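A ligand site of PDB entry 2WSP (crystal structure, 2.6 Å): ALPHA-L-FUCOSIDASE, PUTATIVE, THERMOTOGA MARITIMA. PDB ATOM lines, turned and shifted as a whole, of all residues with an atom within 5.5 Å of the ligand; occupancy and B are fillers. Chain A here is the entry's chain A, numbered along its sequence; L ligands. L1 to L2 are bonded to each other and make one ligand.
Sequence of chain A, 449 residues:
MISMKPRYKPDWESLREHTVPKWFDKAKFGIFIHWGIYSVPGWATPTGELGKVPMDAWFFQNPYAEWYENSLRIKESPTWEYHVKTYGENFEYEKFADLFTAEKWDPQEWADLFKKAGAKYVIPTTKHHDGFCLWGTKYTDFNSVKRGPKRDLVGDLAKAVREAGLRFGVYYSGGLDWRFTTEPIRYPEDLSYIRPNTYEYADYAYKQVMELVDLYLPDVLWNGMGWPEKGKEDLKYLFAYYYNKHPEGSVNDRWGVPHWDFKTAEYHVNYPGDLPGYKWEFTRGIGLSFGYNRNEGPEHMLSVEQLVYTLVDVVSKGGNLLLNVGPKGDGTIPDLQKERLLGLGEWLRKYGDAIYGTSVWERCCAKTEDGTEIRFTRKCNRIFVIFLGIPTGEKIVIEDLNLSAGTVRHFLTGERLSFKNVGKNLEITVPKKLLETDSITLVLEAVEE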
ATOM      1  N   PHE A  32     -11.665  -9.680  27.023  1.00  0.00           N
ATOM      2  CA  PHE A  32     -11.047  -8.669  26.178  1.00  0.00           C
ATOM      3  C   PHE A  32     -11.762  -7.360  26.516  1.00  0.00           C
ATOM      4  O   PHE A  32     -12.967  -7.386  26.759  1.00  0.00           O
ATOM      5  CB  PHE A  32     -11.321  -9.032  24.708  1.00  0.00           C
ATOM      6  CG  PHE A  32     -10.172  -8.801  23.757  1.00  0.00           C
ATOM      7  CD1 PHE A  32      -9.143  -7.911  24.015  1.00  0.00           C
ATOM      8  CD2 PHE A  32     -10.158  -9.475  22.537  1.00  0.00           C
ATOM      9  CE1 PHE A  32      -8.114  -7.723  23.092  1.00  0.00           C
ATOM     10  CE2 PHE A  32      -9.135  -9.295  21.625  1.00  0.00           C
ATOM     11  CZ  PHE A  32      -8.117  -8.421  21.903  1.00  0.00           C
ATOM     12  N   HIS A  34     -12.195  -3.641  24.637  1.00  0.00           N
ATOM     13  CA  HIS A  34     -11.971  -2.571  23.677  1.00  0.00           C
ATOM     14  C   HIS A  34     -12.629  -1.307  24.195  1.00  0.00           C
ATOM     15  O   HIS A  34     -13.848  -1.157  24.148  1.00  0.00           O
ATOM     16  CB  HIS A  34     -12.525  -2.933  22.301  1.00  0.00           C
ATOM     17  CG  HIS A  34     -11.654  -3.882  21.539  1.00  0.00           C
ATOM     18  ND1 HIS A  34     -11.436  -5.180  21.951  1.00  0.00           N
ATOM     19  CD2 HIS A  34     -10.955  -3.730  20.392  1.00  0.00           C
ATOM     20  CE1 HIS A  34     -10.648  -5.784  21.084  1.00  0.00           C
ATOM     21  NE2 HIS A  34     -10.339  -4.931  20.125  1.00  0.00           N
ATOM     22  N   LEU A  50     -17.861 -11.601  10.400  1.00  0.00           N
ATOM     23  CA  LEU A  50     -16.922 -12.000   9.357  1.00  0.00           C
ATOM     24  C   LEU A  50     -17.421 -13.266   8.656  1.00  0.00           C
ATOM     25  O   LEU A  50     -17.791 -14.244   9.318  1.00  0.00           O
ATOM     26  CB  LEU A  50     -15.521 -12.242   9.936  1.00  0.00           C
ATOM     27  CG  LEU A  50     -14.673 -11.015  10.305  1.00  0.00           C
ATOM     28  CD1 LEU A  50     -13.632 -11.382  11.355  1.00  0.00           C
ATOM     29  CD2 LEU A  50     -14.020 -10.388   9.078  1.00  0.00           C
ATOM     30  N   MET A  55     -17.155  -8.716   2.176  1.00  0.00           N
ATOM     31  CA  MET A  55     -15.917  -8.025   2.545  1.00  0.00           C
ATOM     32  C   MET A  55     -15.577  -6.851   1.612  1.00  0.00           C
ATOM     33  O   MET A  55     -14.666  -6.061   1.894  1.00  0.00           O
ATOM     34  CB  MET A  55     -14.743  -9.020   2.575  1.00  0.00           C
ATOM     35  CG  MET A  55     -13.601  -8.630   3.515  1.00  0.00           C
ATOM     36  SD  MET A  55     -14.039  -8.795   5.262  1.00  0.00           S
ATOM     37  CE  MET A  55     -12.575  -8.136   6.069  1.00  0.00           C
ATOM     38  N   TRP A  58     -17.421  -4.115   3.615  1.00  0.00           N
ATOM     39  CA  TRP A  58     -17.159  -4.168   5.063  1.00  0.00           C
ATOM     40  C   TRP A  58     -16.684  -2.845   5.660  1.00  0.00           C
ATOM     41  O   TRP A  58     -17.223  -2.391   6.658  1.00  0.00           O
ATOM     42  CB  TRP A  58     -16.146  -5.274   5.368  1.00  0.00           C
ATOM     43  CG  TRP A  58     -15.778  -5.387   6.826  1.00  0.00           C
ATOM     44  CD1 TRP A  58     -14.778  -4.729   7.481  1.00  0.00           C
ATOM     45  CD2 TRP A  58     -16.414  -6.214   7.816  1.00  0.00           C
ATOM     46  NE1 TRP A  58     -14.752  -5.085   8.808  1.00  0.00           N
ATOM     47  CE2 TRP A  58     -15.749  -6.000   9.037  1.00  0.00           C
ATOM     48  CE3 TRP A  58     -17.491  -7.115   7.788  1.00  0.00           C
ATOM     49  CZ2 TRP A  58     -16.109  -6.656  10.222  1.00  0.00           C
ATOM     50  CZ3 TRP A  58     -17.858  -7.763   8.956  1.00  0.00           C
ATOM     51  CH2 TRP A  58     -17.169  -7.533  10.163  1.00  0.00           C
ATOM     52  N   PHE A  59     -15.663  -2.236   5.055  1.00  0.00           N
ATOM     53  CA  PHE A  59     -15.084  -1.020   5.603  1.00  0.00           C
ATOM     54  C   PHE A  59     -15.989   0.190   5.400  1.00  0.00           C
ATOM     55  O   PHE A  59     -15.922   1.157   6.170  1.00  0.00           O
ATOM     56  CB  PHE A  59     -13.700  -0.756   5.009  1.00  0.00           C
ATOM     57  CG  PHE A  59     -12.705  -1.846   5.318  1.00  0.00           C
ATOM     58  CD1 PHE A  59     -12.153  -1.957   6.592  1.00  0.00           C
ATOM     59  CD2 PHE A  59     -12.346  -2.782   4.360  1.00  0.00           C
ATOM     60  CE1 PHE A  59     -11.248  -2.972   6.891  1.00  0.00           C
ATOM     61  CE2 PHE A  59     -11.444  -3.793   4.651  1.00  0.00           C
ATOM     62  CZ  PHE A  59     -10.893  -3.884   5.912  1.00  0.00           C
ATOM     63  N   ASN A  62     -18.858  -0.549   8.263  1.00  0.00           N
ATOM     64  CA  ASN A  62     -18.086  -1.288   9.267  1.00  0.00           C
ATOM     65  C   ASN A  62     -18.823  -1.505  10.577  1.00  0.00           C
ATOM     66  O   ASN A  62     -19.186  -0.540  11.253  1.00  0.00           O
ATOM     67  CB  ASN A  62     -16.757  -0.574   9.526  1.00  0.00           C
ATOM     68  CG  ASN A  62     -15.691  -1.501  10.099  1.00  0.00           C
ATOM     69  OD1 ASN A  62     -15.988  -2.428  10.851  1.00  0.00           O
ATOM     70  ND2 ASN A  62     -14.442  -1.252   9.734  1.00  0.00           N
ATOM     71  N   TYR A  64     -17.555  -2.738  13.285  1.00  0.00           N
ATOM     72  CA  TYR A  64     -16.636  -2.561  14.416  1.00  0.00           C
ATOM     73  C   TYR A  64     -16.580  -1.080  14.766  1.00  0.00           C
ATOM     74  O   TYR A  64     -16.094  -0.271  13.984  1.00  0.00           O
ATOM     75  CB  TYR A  64     -15.243  -3.077  14.042  1.00  0.00           C
ATOM     76  CG  TYR A  64     -15.100  -4.582  13.907  1.00  0.00           C
ATOM     77  CD1 TYR A  64     -13.858  -5.165  13.683  1.00  0.00           C
ATOM     78  CD2 TYR A  64     -16.205  -5.442  13.994  1.00  0.00           C
ATOM     79  CE1 TYR A  64     -13.708  -6.539  13.538  1.00  0.00           C
ATOM     80  CE2 TYR A  64     -16.067  -6.812  13.856  1.00  0.00           C
ATOM     81  CZ  TYR A  64     -14.818  -7.359  13.635  1.00  0.00           C
ATOM     82  OH  TYR A  64     -14.661  -8.721  13.493  1.00  0.00           O
ATOM     83  N   GLU A  66     -14.883   0.469  16.998  1.00  0.00           N
ATOM     84  CA  GLU A  66     -13.515   0.974  17.221  1.00  0.00           C
ATOM     85  C   GLU A  66     -12.918   1.549  15.932  1.00  0.00           C
ATOM     86  O   GLU A  66     -11.989   2.347  15.995  1.00  0.00           O
ATOM     87  CB  GLU A  66     -12.550  -0.095  17.755  1.00  0.00           C
ATOM     88  CG  GLU A  66     -13.161  -1.338  18.351  1.00  0.00           C
ATOM     89  CD  GLU A  66     -13.569  -2.349  17.285  1.00  0.00           C
ATOM     90  OE1 GLU A  66     -12.693  -3.016  16.720  1.00  0.00           O
ATOM     91  OE2 GLU A  66     -14.775  -2.472  17.039  1.00  0.00           O
ATOM     92  N   TRP A  67     -13.425   1.108  14.784  1.00  0.00           N
ATOM     93  CA  TRP A  67     -12.991   1.616  13.482  1.00  0.00           C
ATOM     94  C   TRP A  67     -13.607   2.965  13.083  1.00  0.00           C
ATOM     95  O   TRP A  67     -13.375   3.439  11.969  1.00  0.00           O
ATOM     96  CB  TRP A  67     -13.262   0.563  12.397  1.00  0.00           C
ATOM     97  CG  TRP A  67     -12.232  -0.515  12.411  1.00  0.00           C
ATOM     98  CD1 TRP A  67     -12.036  -1.445  13.395  1.00  0.00           C
ATOM     99  CD2 TRP A  67     -11.232  -0.747  11.424  1.00  0.00           C
ATOM    100  NE1 TRP A  67     -10.976  -2.242  13.070  1.00  0.00           N
ATOM    101  CE2 TRP A  67     -10.454  -1.833  11.873  1.00  0.00           C
ATOM    102  CE3 TRP A  67     -10.902  -0.140  10.204  1.00  0.00           C
ATOM    103  CZ2 TRP A  67      -9.385  -2.340  11.127  1.00  0.00           C
ATOM    104  CZ3 TRP A  67      -9.841  -0.646   9.473  1.00  0.00           C
ATOM    105  CH2 TRP A  67      -9.093  -1.736   9.932  1.00  0.00           C
ATOM    106  N   HIS A 128      -5.245   1.149  20.475  1.00  0.00           N
ATOM    107  CA  HIS A 128      -5.844   0.530  19.313  1.00  0.00           C
ATOM    108  C   HIS A 128      -5.380   1.262  18.038  1.00  0.00           C
ATOM    109  O   HIS A 128      -4.367   1.977  18.061  1.00  0.00           O
ATOM    110  CB  HIS A 128      -7.372   0.538  19.457  1.00  0.00           C
ATOM    111  CG  HIS A 128      -8.053  -0.533  18.666  1.00  0.00           C
ATOM    112  ND1 HIS A 128      -8.729  -0.269  17.496  1.00  0.00           N
ATOM    113  CD2 HIS A 128      -8.104  -1.880  18.846  1.00  0.00           C
ATOM    114  CE1 HIS A 128      -9.179  -1.401  16.995  1.00  0.00           C
ATOM    115  NE2 HIS A 128      -8.826  -2.391  17.801  1.00  0.00           N
ATOM    116  N   HIS A 129      -6.077   1.069  16.925  1.00  0.00           N
ATOM    117  CA  HIS A 129      -5.662   1.606  15.645  1.00  0.00           C
ATOM    118  C   HIS A 129      -5.640   3.137  15.605  1.00  0.00           C
ATOM    119  O   HIS A 129      -4.791   3.723  14.931  1.00  0.00           O
ATOM    120  CB  HIS A 129      -6.535   1.068  14.508  1.00  0.00           C
ATOM    121  CG  HIS A 129      -6.660  -0.432  14.487  1.00  0.00           C
ATOM    122  ND1 HIS A 129      -5.683  -1.256  15.005  1.00  0.00           N
ATOM    123  CD2 HIS A 129      -7.627  -1.237  14.007  1.00  0.00           C
ATOM    124  CE1 HIS A 129      -6.052  -2.516  14.849  1.00  0.00           C
ATOM    125  NE2 HIS A 129      -7.236  -2.530  14.242  1.00  0.00           N
ATOM    126  N   TYR A 171      -3.360  -5.565  25.284  1.00  0.00           N
ATOM    127  CA  TYR A 171      -3.519  -5.468  23.838  1.00  0.00           C
ATOM    128  C   TYR A 171      -2.807  -4.206  23.340  1.00  0.00           C
ATOM    129  O   TYR A 171      -3.001  -3.125  23.895  1.00  0.00           O
ATOM    130  CB  TYR A 171      -4.990  -5.417  23.432  1.00  0.00           C
ATOM    131  CG  TYR A 171      -5.185  -5.127  21.952  1.00  0.00           C
ATOM    132  CD1 TYR A 171      -5.122  -3.826  21.460  1.00  0.00           C
ATOM    133  CD2 TYR A 171      -5.383  -6.161  21.049  1.00  0.00           C
ATOM    134  CE1 TYR A 171      -5.265  -3.566  20.112  1.00  0.00           C
ATOM    135  CE2 TYR A 171      -5.536  -5.910  19.689  1.00  0.00           C
ATOM    136  CZ  TYR A 171      -5.477  -4.608  19.234  1.00  0.00           C
ATOM    137  OH  TYR A 171      -5.629  -4.328  17.887  1.00  0.00           O
ATOM    138  N   TRP A 222      -0.567  -9.173  23.667  1.00  0.00           N
ATOM    139  CA  TRP A 222      -1.529  -9.476  22.599  1.00  0.00           C
ATOM    140  C   TRP A 222      -1.444  -8.388  21.540  1.00  0.00           C
ATOM    141  O   TRP A 222      -1.984  -7.305  21.704  1.00  0.00           O
ATOM    142  CB  TRP A 222      -2.947  -9.515  23.186  1.00  0.00           C
ATOM    143  CG  TRP A 222      -3.919 -10.468  22.528  1.00  0.00           C
ATOM    144  CD1 TRP A 222      -4.383 -11.653  23.044  1.00  0.00           C
ATOM    145  CD2 TRP A 222      -4.581 -10.302  21.268  1.00  0.00           C
ATOM    146  NE1 TRP A 222      -5.276 -12.226  22.171  1.00  0.00           N
ATOM    147  CE2 TRP A 222      -5.418 -11.420  21.080  1.00  0.00           C
ATOM    148  CE3 TRP A 222      -4.541  -9.306  20.277  1.00  0.00           C
ATOM    149  CZ2 TRP A 222      -6.213 -11.578  19.941  1.00  0.00           C
ATOM    150  CZ3 TRP A 222      -5.336  -9.465  19.138  1.00  0.00           C
ATOM    151  CH2 TRP A 222      -6.159 -10.599  18.984  1.00  0.00           C
ATOM    152  N   MET A 225      -2.825  -6.780  14.227  1.00  0.00           N
ATOM    153  CA  MET A 225      -2.558  -6.323  12.864  1.00  0.00           C
ATOM    154  C   MET A 225      -1.090  -6.428  12.435  1.00  0.00           C
ATOM    155  O   MET A 225      -0.631  -5.671  11.567  1.00  0.00           O
ATOM    156  CB  MET A 225      -3.093  -4.890  12.663  1.00  0.00           C
ATOM    157  CG  MET A 225      -4.608  -4.800  12.723  1.00  0.00           C
ATOM    158  SD  MET A 225      -5.395  -5.633  11.321  1.00  0.00           S
ATOM    159  CE  MET A 225      -4.717  -4.700   9.947  1.00  0.00           C
ATOM    160  N   ARG A 254       0.127 -12.715  16.245  1.00  0.00           N
ATOM    161  CA  ARG A 254      -0.209 -11.689  15.272  1.00  0.00           C
ATOM    162  C   ARG A 254       0.903 -10.653  15.162  1.00  0.00           C
ATOM    163  O   ARG A 254       0.640  -9.461  15.014  1.00  0.00           O
ATOM    164  CB  ARG A 254      -1.526 -11.031  15.672  1.00  0.00           C
ATOM    165  CG  ARG A 254      -2.695 -12.013  15.726  1.00  0.00           C
ATOM    166  CD  ARG A 254      -4.010 -11.253  15.806  1.00  0.00           C
ATOM    167  NE  ARG A 254      -5.165 -12.158  15.880  1.00  0.00           N
ATOM    168  CZ  ARG A 254      -6.424 -11.803  15.642  1.00  0.00           C
ATOM    169  NH1 ARG A 254      -6.741 -10.549  15.309  1.00  0.00           N
ATOM    170  NH2 ARG A 254      -7.386 -12.702  15.745  1.00  0.00           N
ATOM    171  N   GLU A 266     -10.547 -15.919  14.793  1.00  0.00           N
ATOM    172  CA  GLU A 266     -11.678 -15.007  14.800  1.00  0.00           C
ATOM    173  C   GLU A 266     -12.780 -15.471  13.842  1.00  0.00           C
ATOM    174  O   GLU A 266     -13.552 -14.663  13.314  1.00  0.00           O
ATOM    175  CB  GLU A 266     -11.199 -13.565  14.524  1.00  0.00           C
ATOM    176  CG  GLU A 266      -9.919 -13.438  13.669  1.00  0.00           C
ATOM    177  CD  GLU A 266     -10.155 -13.667  12.178  1.00  0.00           C
ATOM    178  OE1 GLU A 266      -9.281 -14.293  11.526  1.00  0.00           O
ATOM    179  OE2 GLU A 266     -11.196 -13.209  11.649  1.00  0.00           O
ATOM    180  N   THR A 283     -11.487 -15.472  19.863  1.00  0.00           N
ATOM    181  CA  THR A 283     -11.869 -14.147  20.343  1.00  0.00           C
ATOM    182  C   THR A 283     -13.119 -13.674  19.588  1.00  0.00           C
ATOM    183  O   THR A 283     -13.196 -13.807  18.375  1.00  0.00           O
ATOM    184  CB  THR A 283     -10.717 -13.132  20.170  1.00  0.00           C
ATOM    185  OG1 THR A 283     -11.002 -11.936  20.903  1.00  0.00           O
ATOM    186  CG2 THR A 283     -10.480 -12.781  18.707  1.00  0.00           C
ATOM    187  N   PHE A 290     -16.444  -4.896  18.687  1.00  0.00           N
ATOM    188  CA  PHE A 290     -15.619  -5.007  19.883  1.00  0.00           C
ATOM    189  C   PHE A 290     -15.803  -3.771  20.760  1.00  0.00           C
ATOM    190  O   PHE A 290     -15.990  -3.899  21.967  1.00  0.00           O
ATOM    191  CB  PHE A 290     -14.150  -5.186  19.513  1.00  0.00           C
ATOM    192  CG  PHE A 290     -13.847  -6.521  18.894  1.00  0.00           C
ATOM    193  CD1 PHE A 290     -14.053  -6.730  17.543  1.00  0.00           C
ATOM    194  CD2 PHE A 290     -13.365  -7.570  19.663  1.00  0.00           C
ATOM    195  CE1 PHE A 290     -13.776  -7.963  16.961  1.00  0.00           C
ATOM    196  CE2 PHE A 290     -13.093  -8.812  19.092  1.00  0.00           C
ATOM    197  CZ  PHE A 290     -13.296  -9.004  17.736  1.00  0.00           C
HETATM  198  C1  LIG L   1      -9.915  -7.383  11.269  1.00  0.00           C
HETATM  199  N1  LIG L   1      -9.756  -5.932  11.405  1.00  0.00           N
HETATM  200  C2  LIG L   1      -9.521  -8.083  12.569  1.00  0.00           C
HETATM  201  N2  LIG L   1     -10.759  -5.197  11.271  1.00  0.00           N
HETATM  202  O1  LIG L   1      -9.978  -7.427  13.751  1.00  0.00           O
HETATM  203  C3  LIG L   1     -10.095  -9.491  12.449  1.00  0.00           C
HETATM  204  N3  LIG L   1     -11.794  -4.519  11.134  1.00  0.00           N
HETATM  205  O2  LIG L   1      -9.883 -10.221  13.668  1.00  0.00           O
HETATM  206  C4  LIG L   1      -9.437 -10.183  11.248  1.00  0.00           C
HETATM  207  O3  LIG L   1      -8.100 -10.547  11.580  1.00  0.00           O
HETATM  208  C5  LIG L   1      -9.412  -9.309   9.977  1.00  0.00           C
HETATM  209  O4  LIG L   1      -9.079  -7.939  10.251  1.00  0.00           O
HETATM  210  C6  LIG L   1      -8.413  -9.880   8.967  1.00  0.00           C
HETATM  211  C1  LG2 L   2      -8.931  -6.937  14.602  1.00  0.00           C
HETATM  212  C2  LG2 L   2      -9.097  -5.432  14.842  1.00  0.00           C
HETATM  213  C3  LG2 L   2     -10.364  -5.167  15.623  1.00  0.00           C
HETATM  214  C4  LG2 L   2     -10.348  -5.935  16.941  1.00  0.00           C
HETATM  215  C5  LG2 L   2     -10.096  -7.421  16.675  1.00  0.00           C
HETATM  216  C6  LG2 L   2      -9.926  -8.163  17.988  1.00  0.00           C
HETATM  217  O1  LG2 L   2      -9.125  -4.692  13.622  1.00  0.00           O
HETATM  218  O2  LG2 L   2     -10.471  -3.769  15.869  1.00  0.00           O
HETATM  219  O3  LG2 L   2      -9.319  -5.409  17.782  1.00  0.00           O
HETATM  220  O4  LG2 L   2      -8.939  -7.627  15.861  1.00  0.00           O
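O3 of LG2 L2 sits at hydrogen-bond distance from NE2 of His 34, 2.6 Å away.
NE2 of His 129 sits at hydrogen-bond distance from O1 of LG2 L2, 2.9 Å away.
An oxygen (O2) of LG2 L2 is in hydrogen-bond range of a ring nitrogen (NE2) of His 128, 2.9 Å away.
The indole nitrogen (NE1) of Trp 67 is in hydrogen-bond range of an oxygen (O1) of LG2 L2 (3.1 Å).
The side-chain carboxylate (OE1) of Glu 66 lies within hydrogen-bond range of an oxygen (O2) of LG2 L2, at 2.5 Å.
The side-chain carboxylate (OE2) of Glu 66 sits at hydrogen-bond distance from the backbone NH (N) of Phe 290 (3.4 Å).
OD1 of Asn 62 is in hydrogen-bond range of N of Tyr 64 (2.9 Å).
CE2 of Phe 32 touches C6 of LG2 L2, 3.9 Å away.
NE1 of Trp 58 touches N3 of LIG L1 (3.8 Å).
CD1 of Tyr 64 touches N3 of LIG L1, at 3.3 Å.
OH of Tyr 171 touches O3 of LG2 L2, 3.8 Å away.
NH1 of Arg 254 touches O2 of LIG L1 (3.6 Å).
CG of Glu 266 touches O2 of LIG L1 (3.2 Å).
Phe 290 touches the ligand.
Within 4 Å of the ligand: Phe 32, His 34, Trp 58, Tyr 64, Glu 66, Trp 67, His 128, His 129, Tyr 171, Arg 254, Glu 266 and Phe 290.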
